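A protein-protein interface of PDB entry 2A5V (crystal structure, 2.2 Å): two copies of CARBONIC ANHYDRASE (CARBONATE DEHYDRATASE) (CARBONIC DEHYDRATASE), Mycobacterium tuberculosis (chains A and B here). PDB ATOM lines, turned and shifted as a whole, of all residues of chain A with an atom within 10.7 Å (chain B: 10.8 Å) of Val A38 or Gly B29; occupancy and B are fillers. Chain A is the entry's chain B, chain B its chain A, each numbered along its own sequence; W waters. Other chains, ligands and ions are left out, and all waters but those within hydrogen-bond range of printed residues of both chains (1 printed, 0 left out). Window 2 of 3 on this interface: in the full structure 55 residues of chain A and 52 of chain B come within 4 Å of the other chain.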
ATOM      1  N   HIS A  33     -38.650   5.820   3.952  1.00  0.00           N
ATOM      2  CA  HIS A  33     -37.298   5.251   3.797  1.00  0.00           C
ATOM      3  C   HIS A  33     -36.224   6.366   3.741  1.00  0.00           C
ATOM      4  O   HIS A  33     -35.442   6.449   2.779  1.00  0.00           O
ATOM      5  CB  HIS A  33     -37.248   4.345   2.557  1.00  0.00           C
ATOM      6  CG  HIS A  33     -38.141   3.148   2.675  1.00  0.00           C
ATOM      7  ND1 HIS A  33     -39.189   2.901   1.808  1.00  0.00           N
ATOM      8  CD2 HIS A  33     -38.161   2.150   3.586  1.00  0.00           C
ATOM      9  CE1 HIS A  33     -39.809   1.799   2.172  1.00  0.00           C
ATOM     10  NE2 HIS A  33     -39.205   1.323   3.252  1.00  0.00           N
ATOM     11  N   PRO A  34     -36.207   7.249   4.770  1.00  0.00           N
ATOM     12  CA  PRO A  34     -35.383   8.469   4.619  1.00  0.00           C
ATOM     13  C   PRO A  34     -33.906   8.150   4.856  1.00  0.00           C
ATOM     14  O   PRO A  34     -33.592   7.058   5.334  1.00  0.00           O
ATOM     15  CB  PRO A  34     -35.929   9.388   5.713  1.00  0.00           C
ATOM     16  CG  PRO A  34     -36.392   8.404   6.817  1.00  0.00           C
ATOM     17  CD  PRO A  34     -36.924   7.207   6.067  1.00  0.00           C
ATOM     18  N   SER A  35     -33.022   9.084   4.497  1.00  0.00           N
ATOM     19  CA  SER A  35     -31.602   9.006   4.848  1.00  0.00           C
ATOM     20  C   SER A  35     -30.891   7.711   4.431  1.00  0.00           C
ATOM     21  O   SER A  35     -30.119   7.158   5.216  1.00  0.00           O
ATOM     22  CB  SER A  35     -31.427   9.190   6.370  1.00  0.00           C
ATOM     23  OG  SER A  35     -31.902  10.470   6.749  1.00  0.00           O
ATOM     24  N   GLN A  36     -31.155   7.241   3.211  1.00  0.00           N
ATOM     25  CA  GLN A  36     -30.450   6.071   2.679  1.00  0.00           C
ATOM     26  C   GLN A  36     -30.163   6.118   1.167  1.00  0.00           C
ATOM     27  O   GLN A  36     -29.947   5.084   0.525  1.00  0.00           O
ATOM     28  CB  GLN A  36     -31.147   4.771   3.109  1.00  0.00           C
ATOM     29  CG  GLN A  36     -32.572   4.644   2.681  1.00  0.00           C
ATOM     30  CD  GLN A  36     -33.358   3.735   3.605  1.00  0.00           C
ATOM     31  OE1 GLN A  36     -33.602   2.567   3.279  1.00  0.00           O
ATOM     32  NE2 GLN A  36     -33.771   4.267   4.759  1.00  0.00           N
ATOM     33  N   SER A  37     -30.154   7.323   0.605  1.00  0.00           N
ATOM     34  CA  SER A  37     -29.800   7.503  -0.795  1.00  0.00           C
ATOM     35  C   SER A  37     -28.292   7.340  -0.918  1.00  0.00           C
ATOM     36  O   SER A  37     -27.566   7.440   0.084  1.00  0.00           O
ATOM     37  CB  SER A  37     -30.228   8.882  -1.299  1.00  0.00           C
ATOM     38  OG  SER A  37     -29.364   9.895  -0.813  1.00  0.00           O
ATOM     39  N   VAL A  38     -27.837   7.072  -2.139  1.00  0.00           N
ATOM     40  CA  VAL A  38     -26.412   6.925  -2.456  1.00  0.00           C
ATOM     41  C   VAL A  38     -25.624   8.199  -2.079  1.00  0.00           C
ATOM     42  O   VAL A  38     -24.496   8.107  -1.584  1.00  0.00           O
ATOM     43  CB  VAL A  38     -26.240   6.496  -3.952  1.00  0.00           C
ATOM     44  CG1 VAL A  38     -24.769   6.613  -4.456  1.00  0.00           C
ATOM     45  CG2 VAL A  38     -26.778   5.067  -4.138  1.00  0.00           C
ATOM     46  N   ASP A  39     -26.251   9.365  -2.269  1.00  0.00           N
ATOM     47  CA  ASP A  39     -25.677  10.683  -1.947  1.00  0.00           C
ATOM     48  C   ASP A  39     -25.558  10.950  -0.438  1.00  0.00           C
ATOM     49  O   ASP A  39     -24.500  11.401   0.036  1.00  0.00           O
ATOM     50  CB  ASP A  39     -26.496  11.799  -2.620  1.00  0.00           C
ATOM     51  CG  ASP A  39     -25.888  12.271  -3.959  1.00  0.00           C
ATOM     52  OD1 ASP A  39     -24.638  12.344  -4.077  1.00  0.00           O
ATOM     53  OD2 ASP A  39     -26.660  12.610  -4.893  1.00  0.00           O
ATOM     54  N   HIS A  40     -26.636  10.672   0.307  1.00  0.00           N
ATOM     55  CA  HIS A  40     -26.654  10.839   1.756  1.00  0.00           C
ATOM     56  C   HIS A  40     -25.684   9.853   2.442  1.00  0.00           C
ATOM     57  O   HIS A  40     -24.964  10.222   3.372  1.00  0.00           O
ATOM     58  CB  HIS A  40     -28.080  10.663   2.305  1.00  0.00           C
ATOM     59  CG  HIS A  40     -28.153  10.676   3.804  1.00  0.00           C
ATOM     60  ND1 HIS A  40     -28.373  11.828   4.530  1.00  0.00           N
ATOM     61  CD2 HIS A  40     -28.032   9.679   4.712  1.00  0.00           C
ATOM     62  CE1 HIS A  40     -28.379  11.539   5.821  1.00  0.00           C
ATOM     63  NE2 HIS A  40     -28.177  10.241   5.956  1.00  0.00           N
ATOM     64  N   ARG A  41     -25.693   8.611   1.947  1.00  0.00           N
ATOM     65  CA  ARG A  41     -24.768   7.537   2.332  1.00  0.00           C
ATOM     66  C   ARG A  41     -23.299   7.948   2.182  1.00  0.00           C
ATOM     67  O   ARG A  41     -22.498   7.754   3.097  1.00  0.00           O
ATOM     68  CB  ARG A  41     -25.065   6.298   1.480  1.00  0.00           C
ATOM     69  CG  ARG A  41     -24.178   5.098   1.705  1.00  0.00           C
ATOM     70  CD  ARG A  41     -24.770   3.889   0.989  1.00  0.00           C
ATOM     71  NE  ARG A  41     -24.254   3.731  -0.370  1.00  0.00           N
ATOM     72  CZ  ARG A  41     -24.883   3.092  -1.353  1.00  0.00           C
ATOM     73  NH1 ARG A  41     -26.077   2.561  -1.159  1.00  0.00           N
ATOM     74  NH2 ARG A  41     -24.314   3.007  -2.549  1.00  0.00           N
ATOM     75  N   ALA A  42     -22.960   8.534   1.037  1.00  0.00           N
ATOM     76  CA  ALA A  42     -21.608   9.030   0.785  1.00  0.00           C
ATOM     77  C   ALA A  42     -21.137  10.079   1.817  1.00  0.00           C
ATOM     78  O   ALA A  42     -19.962  10.093   2.204  1.00  0.00           O
ATOM     79  CB  ALA A  42     -21.504   9.582  -0.642  1.00  0.00           C
ATOM     80  N   GLY A  43     -22.051  10.940   2.268  1.00  0.00           N
ATOM     81  CA  GLY A  43     -21.727  11.963   3.266  1.00  0.00           C
ATOM     82  C   GLY A  43     -21.491  11.423   4.667  1.00  0.00           C
ATOM     83  O   GLY A  43     -21.041  12.151   5.560  1.00  0.00           O
ATOM     84  N   LEU A  44     -21.788  10.143   4.873  1.00  0.00           N
ATOM     85  CA  LEU A  44     -21.671   9.550   6.204  1.00  0.00           C
ATOM     86  C   LEU A  44     -20.288   8.978   6.456  1.00  0.00           C
ATOM     87  O   LEU A  44     -19.916   8.733   7.603  1.00  0.00           O
ATOM     88  CB  LEU A  44     -22.752   8.495   6.444  1.00  0.00           C
ATOM     89  CG  LEU A  44     -24.153   9.047   6.723  1.00  0.00           C
ATOM     90  CD1 LEU A  44     -25.121   7.891   6.768  1.00  0.00           C
ATOM     91  CD2 LEU A  44     -24.223   9.862   8.029  1.00  0.00           C
ATOM     92  N   ALA A  45     -19.522   8.774   5.386  1.00  0.00           N
ATOM     93  CA  ALA A  45     -18.143   8.301   5.528  1.00  0.00           C
ATOM     94  C   ALA A  45     -17.346   9.259   6.434  1.00  0.00           C
ATOM     95  O   ALA A  45     -16.387   8.856   7.095  1.00  0.00           O
ATOM     96  CB  ALA A  45     -17.492   8.160   4.165  1.00  0.00           C
ATOM     97  N   LEU A  72     -29.842   5.657   7.523  1.00  0.00           N
ATOM     98  CA  LEU A  72     -28.467   5.498   7.968  1.00  0.00           C
ATOM     99  C   LEU A  72     -28.049   6.757   8.721  1.00  0.00           C
ATOM    100  O   LEU A  72     -28.477   7.859   8.372  1.00  0.00           O
ATOM    101  CB  LEU A  72     -27.592   5.276   6.742  1.00  0.00           C
ATOM    102  CG  LEU A  72     -28.052   4.127   5.834  1.00  0.00           C
ATOM    103  CD1 LEU A  72     -27.352   4.141   4.489  1.00  0.00           C
ATOM    104  CD2 LEU A  72     -27.851   2.781   6.555  1.00  0.00           C
ATOM    105  N   GLU B  21     -27.334 -10.828  -2.946  1.00  0.00           N
ATOM    106  CA  GLU B  21     -28.286 -10.161  -3.826  1.00  0.00           C
ATOM    107  C   GLU B  21     -28.813  -8.853  -3.237  1.00  0.00           C
ATOM    108  O   GLU B  21     -28.872  -7.838  -3.930  1.00  0.00           O
ATOM    109  CB  GLU B  21     -29.450 -11.091  -4.148  1.00  0.00           C
ATOM    110  CG  GLU B  21     -29.110 -12.213  -5.102  1.00  0.00           C
ATOM    111  CD  GLU B  21     -30.150 -13.314  -5.101  1.00  0.00           C
ATOM    112  OE1 GLU B  21     -30.972 -13.388  -4.139  1.00  0.00           O
ATOM    113  OE2 GLU B  21     -30.129 -14.112  -6.064  1.00  0.00           O
ATOM    114  N   GLY B  22     -29.186  -8.890  -1.956  1.00  0.00           N
ATOM    115  CA  GLY B  22     -29.712  -7.719  -1.272  1.00  0.00           C
ATOM    116  C   GLY B  22     -28.740  -6.549  -1.172  1.00  0.00           C
ATOM    117  O   GLY B  22     -29.138  -5.397  -1.357  1.00  0.00           O
ATOM    118  N   ASN B  23     -27.478  -6.831  -0.835  1.00  0.00           N
ATOM    119  CA  ASN B  23     -26.467  -5.784  -0.798  1.00  0.00           C
ATOM    120  C   ASN B  23     -26.197  -5.216  -2.200  1.00  0.00           C
ATOM    121  O   ASN B  23     -25.820  -4.059  -2.346  1.00  0.00           O
ATOM    122  CB  ASN B  23     -25.165  -6.266  -0.163  1.00  0.00           C
ATOM    123  CG  ASN B  23     -24.132  -5.148  -0.032  1.00  0.00           C
ATOM    124  OD1 ASN B  23     -23.047  -5.209  -0.618  1.00  0.00           O
ATOM    125  ND2 ASN B  23     -24.476  -4.114   0.726  1.00  0.00           N
ATOM    126  N   GLU B  24     -26.406  -6.035  -3.226  1.00  0.00           N
ATOM    127  CA  GLU B  24     -26.248  -5.579  -4.603  1.00  0.00           C
ATOM    128  C   GLU B  24     -27.288  -4.551  -4.996  1.00  0.00           C
ATOM    129  O   GLU B  24     -26.965  -3.578  -5.656  1.00  0.00           O
ATOM    130  CB  GLU B  24     -26.241  -6.754  -5.570  1.00  0.00           C
ATOM    131  CG  GLU B  24     -24.959  -7.570  -5.451  1.00  0.00           C
ATOM    132  CD  GLU B  24     -24.983  -8.859  -6.266  1.00  0.00           C
ATOM    133  OE1 GLU B  24     -25.892  -9.010  -7.127  1.00  0.00           O
ATOM    134  OE2 GLU B  24     -24.075  -9.706  -6.038  1.00  0.00           O
ATOM    135  N   ARG B  25     -28.526  -4.732  -4.547  1.00  0.00           N
ATOM    136  CA  ARG B  25     -29.584  -3.766  -4.863  1.00  0.00           C
ATOM    137  C   ARG B  25     -29.312  -2.478  -4.098  1.00  0.00           C
ATOM    138  O   ARG B  25     -29.469  -1.389  -4.638  1.00  0.00           O
ATOM    139  CB  ARG B  25     -30.967  -4.300  -4.489  1.00  0.00           C
ATOM    140  CG  ARG B  25     -31.293  -5.663  -5.058  1.00  0.00           C
ATOM    141  CD  ARG B  25     -32.742  -6.021  -4.776  1.00  0.00           C
ATOM    142  NE  ARG B  25     -32.985  -6.392  -3.394  1.00  0.00           N
ATOM    143  CZ  ARG B  25     -32.888  -7.631  -2.921  1.00  0.00           C
ATOM    144  NH1 ARG B  25     -32.538  -8.636  -3.720  1.00  0.00           N
ATOM    145  NH2 ARG B  25     -33.132  -7.862  -1.635  1.00  0.00           N
ATOM    146  N   PHE B  26     -28.894  -2.623  -2.842  1.00  0.00           N
ATOM    147  CA  PHE B  26     -28.491  -1.485  -2.029  1.00  0.00           C
ATOM    148  C   PHE B  26     -27.357  -0.697  -2.668  1.00  0.00           C
ATOM    149  O   PHE B  26     -27.469   0.512  -2.806  1.00  0.00           O
ATOM    150  CB  PHE B  26     -28.067  -1.929  -0.625  1.00  0.00           C
ATOM    151  CG  PHE B  26     -27.643  -0.798   0.268  1.00  0.00           C
ATOM    152  CD1 PHE B  26     -28.575   0.132   0.724  1.00  0.00           C
ATOM    153  CD2 PHE B  26     -26.318  -0.669   0.667  1.00  0.00           C
ATOM    154  CE1 PHE B  26     -28.195   1.176   1.584  1.00  0.00           C
ATOM    155  CE2 PHE B  26     -25.918   0.369   1.540  1.00  0.00           C
ATOM    156  CZ  PHE B  26     -26.870   1.297   1.994  1.00  0.00           C
ATOM    157  N   VAL B  27     -26.269  -1.380  -3.038  1.00  0.00           N
ATOM    158  CA  VAL B  27     -25.137  -0.740  -3.721  1.00  0.00           C
ATOM    159  C   VAL B  27     -25.559   0.038  -4.984  1.00  0.00           C
ATOM    160  O   VAL B  27     -25.113   1.178  -5.195  1.00  0.00           O
ATOM    161  CB  VAL B  27     -24.031  -1.769  -4.079  1.00  0.00           C
ATOM    162  CG1 VAL B  27     -23.002  -1.163  -5.019  1.00  0.00           C
ATOM    163  CG2 VAL B  27     -23.367  -2.301  -2.807  1.00  0.00           C
ATOM    164  N   ALA B  28     -26.419  -0.575  -5.801  1.00  0.00           N
ATOM    165  CA  ALA B  28     -26.858   0.018  -7.066  1.00  0.00           C
ATOM    166  C   ALA B  28     -27.928   1.084  -6.872  1.00  0.00           C
ATOM    167  O   ALA B  28     -28.413   1.638  -7.843  1.00  0.00           O
ATOM    168  CB  ALA B  28     -27.347  -1.062  -8.035  1.00  0.00           C
ATOM    169  N   GLY B  29     -28.289   1.371  -5.619  1.00  0.00           N
ATOM    170  CA  GLY B  29     -29.330   2.360  -5.315  1.00  0.00           C
ATOM    171  C   GLY B  29     -30.700   1.889  -5.759  1.00  0.00           C
ATOM    172  O   GLY B  29     -31.567   2.708  -6.090  1.00  0.00           O
ATOM    173  N   ARG B  30     -30.900   0.569  -5.779  1.00  0.00           N
ATOM    174  CA  ARG B  30     -32.174  -0.023  -6.259  1.00  0.00           C
ATOM    175  C   ARG B  30     -32.871  -0.899  -5.210  1.00  0.00           C
ATOM    176  O   ARG B  30     -33.245  -2.040  -5.528  1.00  0.00           O
ATOM    177  CB  ARG B  30     -31.954  -0.863  -7.534  1.00  0.00           C
ATOM    178  CG  ARG B  30     -31.179  -0.172  -8.626  1.00  0.00           C
ATOM    179  CD  ARG B  30     -32.066   0.781  -9.364  1.00  0.00           C
ATOM    180  NE  ARG B  30     -31.522   2.131  -9.293  1.00  0.00           N
ATOM    181  CZ  ARG B  30     -32.014   3.171  -9.956  1.00  0.00           C
ATOM    182  NH1 ARG B  30     -33.066   3.015 -10.754  1.00  0.00           N
ATOM    183  NH2 ARG B  30     -31.450   4.367  -9.819  1.00  0.00           N
ATOM    184  N   PRO B  31     -33.101  -0.360  -3.985  1.00  0.00           N
ATOM    185  CA  PRO B  31     -33.605  -1.236  -2.927  1.00  0.00           C
ATOM    186  C   PRO B  31     -35.068  -1.557  -3.191  1.00  0.00           C
ATOM    187  O   PRO B  31     -35.795  -0.713  -3.701  1.00  0.00           O
ATOM    188  CB  PRO B  31     -33.450  -0.401  -1.652  1.00  0.00           C
ATOM    189  CG  PRO B  31     -33.301   1.013  -2.099  1.00  0.00           C
ATOM    190  CD  PRO B  31     -32.996   1.050  -3.549  1.00  0.00           C
ATOM    191  N   GLN B  32     -35.482  -2.784  -2.884  1.00  0.00           N
ATOM    192  CA  GLN B  32     -36.876  -3.166  -3.075  1.00  0.00           C
ATOM    193  C   GLN B  32     -37.625  -3.017  -1.763  1.00  0.00           C
ATOM    194  O   GLN B  32     -38.837  -3.039  -1.749  1.00  0.00           O
ATOM    195  CB  GLN B  32     -36.979  -4.597  -3.599  1.00  0.00           C
ATOM    196  CG  GLN B  32     -36.801  -4.722  -5.119  1.00  0.00           C
ATOM    197  CD  GLN B  32     -36.230  -6.076  -5.562  1.00  0.00           C
ATOM    198  OE1 GLN B  32     -36.278  -7.068  -4.824  1.00  0.00           O
ATOM    199  NE2 GLN B  32     -35.671  -6.110  -6.776  1.00  0.00           N
ATOM    200  N   HIS B  33     -36.892  -2.862  -0.658  1.00  0.00           N
ATOM    201  CA  HIS B  33     -37.487  -2.807   0.687  1.00  0.00           C
ATOM    202  C   HIS B  33     -38.503  -3.935   0.881  1.00  0.00           C
ATOM    203  O   HIS B  33     -39.668  -3.666   1.115  1.00  0.00           O
ATOM    204  CB  HIS B  33     -38.157  -1.442   0.918  1.00  0.00           C
ATOM    205  CG  HIS B  33     -37.193  -0.296   0.925  1.00  0.00           C
ATOM    206  ND1 HIS B  33     -37.155   0.649  -0.078  1.00  0.00           N
ATOM    207  CD2 HIS B  33     -36.226   0.052   1.810  1.00  0.00           C
ATOM    208  CE1 HIS B  33     -36.212   1.534   0.192  1.00  0.00           C
ATOM    209  NE2 HIS B  33     -35.629   1.192   1.328  1.00  0.00           N
ATOM    210  N   ILE B  66     -30.996  -2.565   6.207  1.00  0.00           N
ATOM    211  CA  ILE B  66     -31.001  -1.586   5.129  1.00  0.00           C
ATOM    212  C   ILE B  66     -29.868  -1.923   4.157  1.00  0.00           C
ATOM    213  O   ILE B  66     -30.087  -2.051   2.950  1.00  0.00           O
ATOM    214  CB  ILE B  66     -30.861  -0.124   5.657  1.00  0.00           C
ATOM    215  CG1 ILE B  66     -32.029   0.239   6.585  1.00  0.00           C
ATOM    216  CG2 ILE B  66     -30.752   0.890   4.480  1.00  0.00           C
ATOM    217  CD1 ILE B  66     -32.075   1.742   6.981  1.00  0.00           C
ATOM    218  N   ILE B  67     -28.662  -2.104   4.692  1.00  0.00           N
ATOM    219  CA  ILE B  67     -27.517  -2.375   3.826  1.00  0.00           C
ATOM    220  C   ILE B  67     -27.577  -3.701   2.999  1.00  0.00           C
ATOM    221  O   ILE B  67     -26.963  -3.805   1.950  1.00  0.00           O
ATOM    222  CB  ILE B  67     -26.183  -2.149   4.564  1.00  0.00           C
ATOM    223  CG1 ILE B  67     -25.888  -3.286   5.541  1.00  0.00           C
ATOM    224  CG2 ILE B  67     -26.195  -0.772   5.220  1.00  0.00           C
ATOM    225  CD1 ILE B  67     -24.603  -3.114   6.306  1.00  0.00           C
ATOM    226  N   ASP B  69     -30.629  -4.906   2.126  1.00  0.00           N
ATOM    227  CA  ASP B  69     -32.001  -4.803   1.553  1.00  0.00           C
ATOM    228  C   ASP B  69     -32.890  -6.006   1.939  1.00  0.00           C
ATOM    229  O   ASP B  69     -33.526  -6.627   1.067  1.00  0.00           O
ATOM    230  CB  ASP B  69     -31.962  -4.560   0.031  1.00  0.00           C
ATOM    231  CG  ASP B  69     -33.298  -4.046  -0.544  1.00  0.00           C
ATOM    232  OD1 ASP B  69     -34.023  -3.286   0.140  1.00  0.00           O
ATOM    233  OD2 ASP B  69     -33.618  -4.404  -1.703  1.00  0.00           O
ATOM    234  N   TYR B 193     -18.170  -3.913   5.765  1.00  0.00           N
ATOM    235  CA  TYR B 193     -18.995  -2.955   5.052  1.00  0.00           C
ATOM    236  C   TYR B 193     -18.201  -1.700   4.727  1.00  0.00           C
ATOM    237  O   TYR B 193     -17.451  -1.209   5.551  1.00  0.00           O
ATOM    238  CB  TYR B 193     -20.241  -2.617   5.874  1.00  0.00           C
ATOM    239  CG  TYR B 193     -21.133  -1.532   5.295  1.00  0.00           C
ATOM    240  CD1 TYR B 193     -21.953  -1.786   4.201  1.00  0.00           C
ATOM    241  CD2 TYR B 193     -21.164  -0.256   5.869  1.00  0.00           C
ATOM    242  CE1 TYR B 193     -22.788  -0.794   3.684  1.00  0.00           C
ATOM    243  CE2 TYR B 193     -21.977   0.734   5.371  1.00  0.00           C
ATOM    244  CZ  TYR B 193     -22.788   0.471   4.266  1.00  0.00           C
ATOM    245  OH  TYR B 193     -23.612   1.468   3.782  1.00  0.00           O
ATOM    246  N   GLN B 194     -18.380  -1.186   3.524  1.00  0.00           N
ATOM    247  CA  GLN B 194     -17.672   0.012   3.064  1.00  0.00           C
ATOM    248  C   GLN B 194     -18.614   1.200   3.049  1.00  0.00           C
ATOM    249  O   GLN B 194     -19.584   1.223   2.289  1.00  0.00           O
ATOM    250  CB  GLN B 194     -17.047  -0.219   1.682  1.00  0.00           C
ATOM    251  CG  GLN B 194     -16.110  -1.431   1.650  1.00  0.00           C
ATOM    252  CD  GLN B 194     -15.478  -1.669   0.296  1.00  0.00           C
ATOM    253  OE1 GLN B 194     -15.931  -1.140  -0.730  1.00  0.00           O
ATOM    254  NE2 GLN B 194     -14.430  -2.489   0.281  1.00  0.00           N
ATOM    255  N   LEU B 195     -18.343   2.165   3.919  1.00  0.00           N
ATOM    256  CA  LEU B 195     -19.236   3.302   4.111  1.00  0.00           C
ATOM    257  C   LEU B 195     -19.346   4.182   2.850  1.00  0.00           C
ATOM    258  O   LEU B 195     -20.348   4.871   2.642  1.00  0.00           O
ATOM    259  CB  LEU B 195     -18.781   4.157   5.298  1.00  0.00           C
ATOM    260  CG  LEU B 195     -18.563   3.607   6.716  1.00  0.00           C
ATOM    261  CD1 LEU B 195     -18.220   4.767   7.641  1.00  0.00           C
ATOM    262  CD2 LEU B 195     -19.734   2.843   7.247  1.00  0.00           C
ATOM    263  N   ASP B 196     -18.309   4.138   2.020  1.00  0.00           N
ATOM    264  CA  ASP B 196     -18.234   4.964   0.818  1.00  0.00           C
ATOM    265  C   ASP B 196     -19.258   4.565  -0.205  1.00  0.00           C
ATOM    266  O   ASP B 196     -20.010   5.413  -0.681  1.00  0.00           O
ATOM    267  CB  ASP B 196     -16.848   4.869   0.198  1.00  0.00           C
ATOM    268  CG  ASP B 196     -15.896   5.876   0.778  1.00  0.00           C
ATOM    269  OD1 ASP B 196     -16.143   7.093   0.586  1.00  0.00           O
ATOM    270  OD2 ASP B 196     -14.895   5.460   1.413  1.00  0.00           O
ATOM    271  N   ASP B 197     -19.296   3.274  -0.527  1.00  0.00           N
ATOM    272  CA  ASP B 197     -20.090   2.790  -1.648  1.00  0.00           C
ATOM    273  C   ASP B 197     -21.104   1.738  -1.225  1.00  0.00           C
ATOM    274  O   ASP B 197     -21.866   1.226  -2.045  1.00  0.00           O
ATOM    275  CB  ASP B 197     -19.181   2.288  -2.793  1.00  0.00           C
ATOM    276  CG  ASP B 197     -18.284   1.105  -2.383  1.00  0.00           C
ATOM    277  OD1 ASP B 197     -18.268   0.701  -1.193  1.00  0.00           O
ATOM    278  OD2 ASP B 197     -17.592   0.564  -3.271  1.00  0.00           O
ATOM    279  N   GLY B 198     -21.123   1.426   0.067  1.00  0.00           N
ATOM    280  CA  GLY B 198     -22.133   0.528   0.614  1.00  0.00           C
ATOM    281  C   GLY B 198     -21.970  -0.942   0.276  1.00  0.00           C
ATOM    282  O   GLY B 198     -22.895  -1.710   0.502  1.00  0.00           O
ATOM    283  N   ARG B 199     -20.809  -1.330  -0.259  1.00  0.00           N
ATOM    284  CA  ARG B 199     -20.475  -2.739  -0.534  1.00  0.00           C
ATOM    285  C   ARG B 199     -20.175  -3.537   0.731  1.00  0.00           C
ATOM    286  O   ARG B 199     -19.379  -3.114   1.573  1.00  0.00           O
ATOM    287  CB  ARG B 199     -19.256  -2.865  -1.456  1.00  0.00           C
ATOM    288  CG  ARG B 199     -19.523  -2.501  -2.879  1.00  0.00           C
ATOM    289  CD  ARG B 199     -18.395  -2.961  -3.814  1.00  0.00           C
ATOM    290  NE  ARG B 199     -18.598  -2.413  -5.158  1.00  0.00           N
ATOM    291  CZ  ARG B 199     -19.585  -2.777  -5.983  1.00  0.00           C
ATOM    292  NH1 ARG B 199     -20.482  -3.693  -5.600  1.00  0.00           N
ATOM    293  NH2 ARG B 199     -19.692  -2.211  -7.187  1.00  0.00           N
HETATM  294  O   HOH W   1     -21.699   5.543   4.746  1.00  0.00           O
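NH1 of Arg A41 is in hydrogen-bond range of O of Phe B26, at 3.0 Å. O of Val B27 sits at hydrogen-bond distance from NH2 of Arg A41, at 3.3 Å. The side-chain amide oxygen (OE1) of Gln A36 lies within hydrogen-bond range of a ring nitrogen (NE2) of His B33, 3.1 Å away. The backbone carbonyl oxygen (O) of Asp B197 lies within hydrogen-bond range of the guanidinium group (NH2) of Arg A41 (3.1 Å).
Of the 23 printed residues of chain B, 10 touch a printed residue of chain A. Hydrophobic or aromatic side chains of chain B within 4 Å of the printed part of chain A: Phe B26, His B33, Ile B66 and Tyr B193. Hydrophobic or aromatic side chains of chain A within 4 Å of the printed part of chain B: His A33, Val A38, Ala A45 and Leu A72. Among the printed residues, no Asp or Glu carboxylate lies within 4 Å of a Lys or Arg side-chain nitrogen of the other chain.
His A33 touches its own counterpart, His B33. 1 position is printed for both chains. Of the 12 pairs that touch across the chains among the printed residues, 1 has its exchanged pair printed and touching as well.
Water W1 bridges the backbone carbonyl oxygen (O) of Leu B195 (2.6 Å) and the backbone carbonyl oxygen (O) of Arg A41 (2.9 Å).
The side-chain amide nitrogen of Asn B23 sits at hydrogen-bond distance from the backbone carbonyl oxygen of Gly B198, at 2.9 Å. The side-chain carboxylate (OD1) of Asp B69 lies within hydrogen-bond range of the backbone NH (N) of His B33, 3.0 Å away. OE1 of Gln B194 sits close to OD1 of Asp B197, 3.0 Å away. O of Pro A34 is in hydrogen-bond range of NE2 of Gln A36, at 2.9 Å. N of Leu A72 is in hydrogen-bond range of O of Ser A35 (2.8 Å). A ring nitrogen (NE2) of His A40 is in hydrogen-bond range of the backbone carbonyl oxygen (O) of Leu A72 (3.4 Å).
Gly B29 touches one residue of chain A. Of chain B, only Phe B26, Val B27, Tyr B193, Leu B195, Asp B197 and Gly B198 come within 4 Å of Arg A41. No residue of chain B comes within 4 Å of Ala A42. No residue of chain A comes within 4 Å of Ala B28. No residue of chain A comes within 4 Å of Pro B31. Of the printed residues of chain A, Asp B196 touches Ala A45. Of the printed residues of chain A, Val B27 touches Arg A41. Of the printed residues of chain A, Gly B198 touches Arg A41 (3.9 Å). Of the printed residues of chain A, Leu B195 touches Arg A41. Of the printed residues of chain A, His B33 touches His A33 and Gln A36. Gly B22 touches none of the printed residues of chain A. The nearest residue of chain B that does not touch Val A38 is Val B27 (4.4 Å). The nearest residue of chain A that does not touch Gly B29 is Arg A41 (5.1 Å). The nearest printed residue of chain B that does not touch Gln A36 is Phe B26 (4.4 Å).
CD2 of His A33 touches CD2 of His B33, at 3.4 Å. Gln A36 touches Ile B66 (OE1 to CG2, 3.5 Å). Val A38 touches Gly B29. Arg A41 touches Tyr B193 (CD to OH, 3.9 Å). Arg A41 touches Leu B195 (O to O, 3.6 Å). Arg A41 touches Gly B198 (NE to N, 3.9 Å). Ala A45 touches Asp B196 (CB to OD1, 3.97 Å). Phe B26 touches Leu A72.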
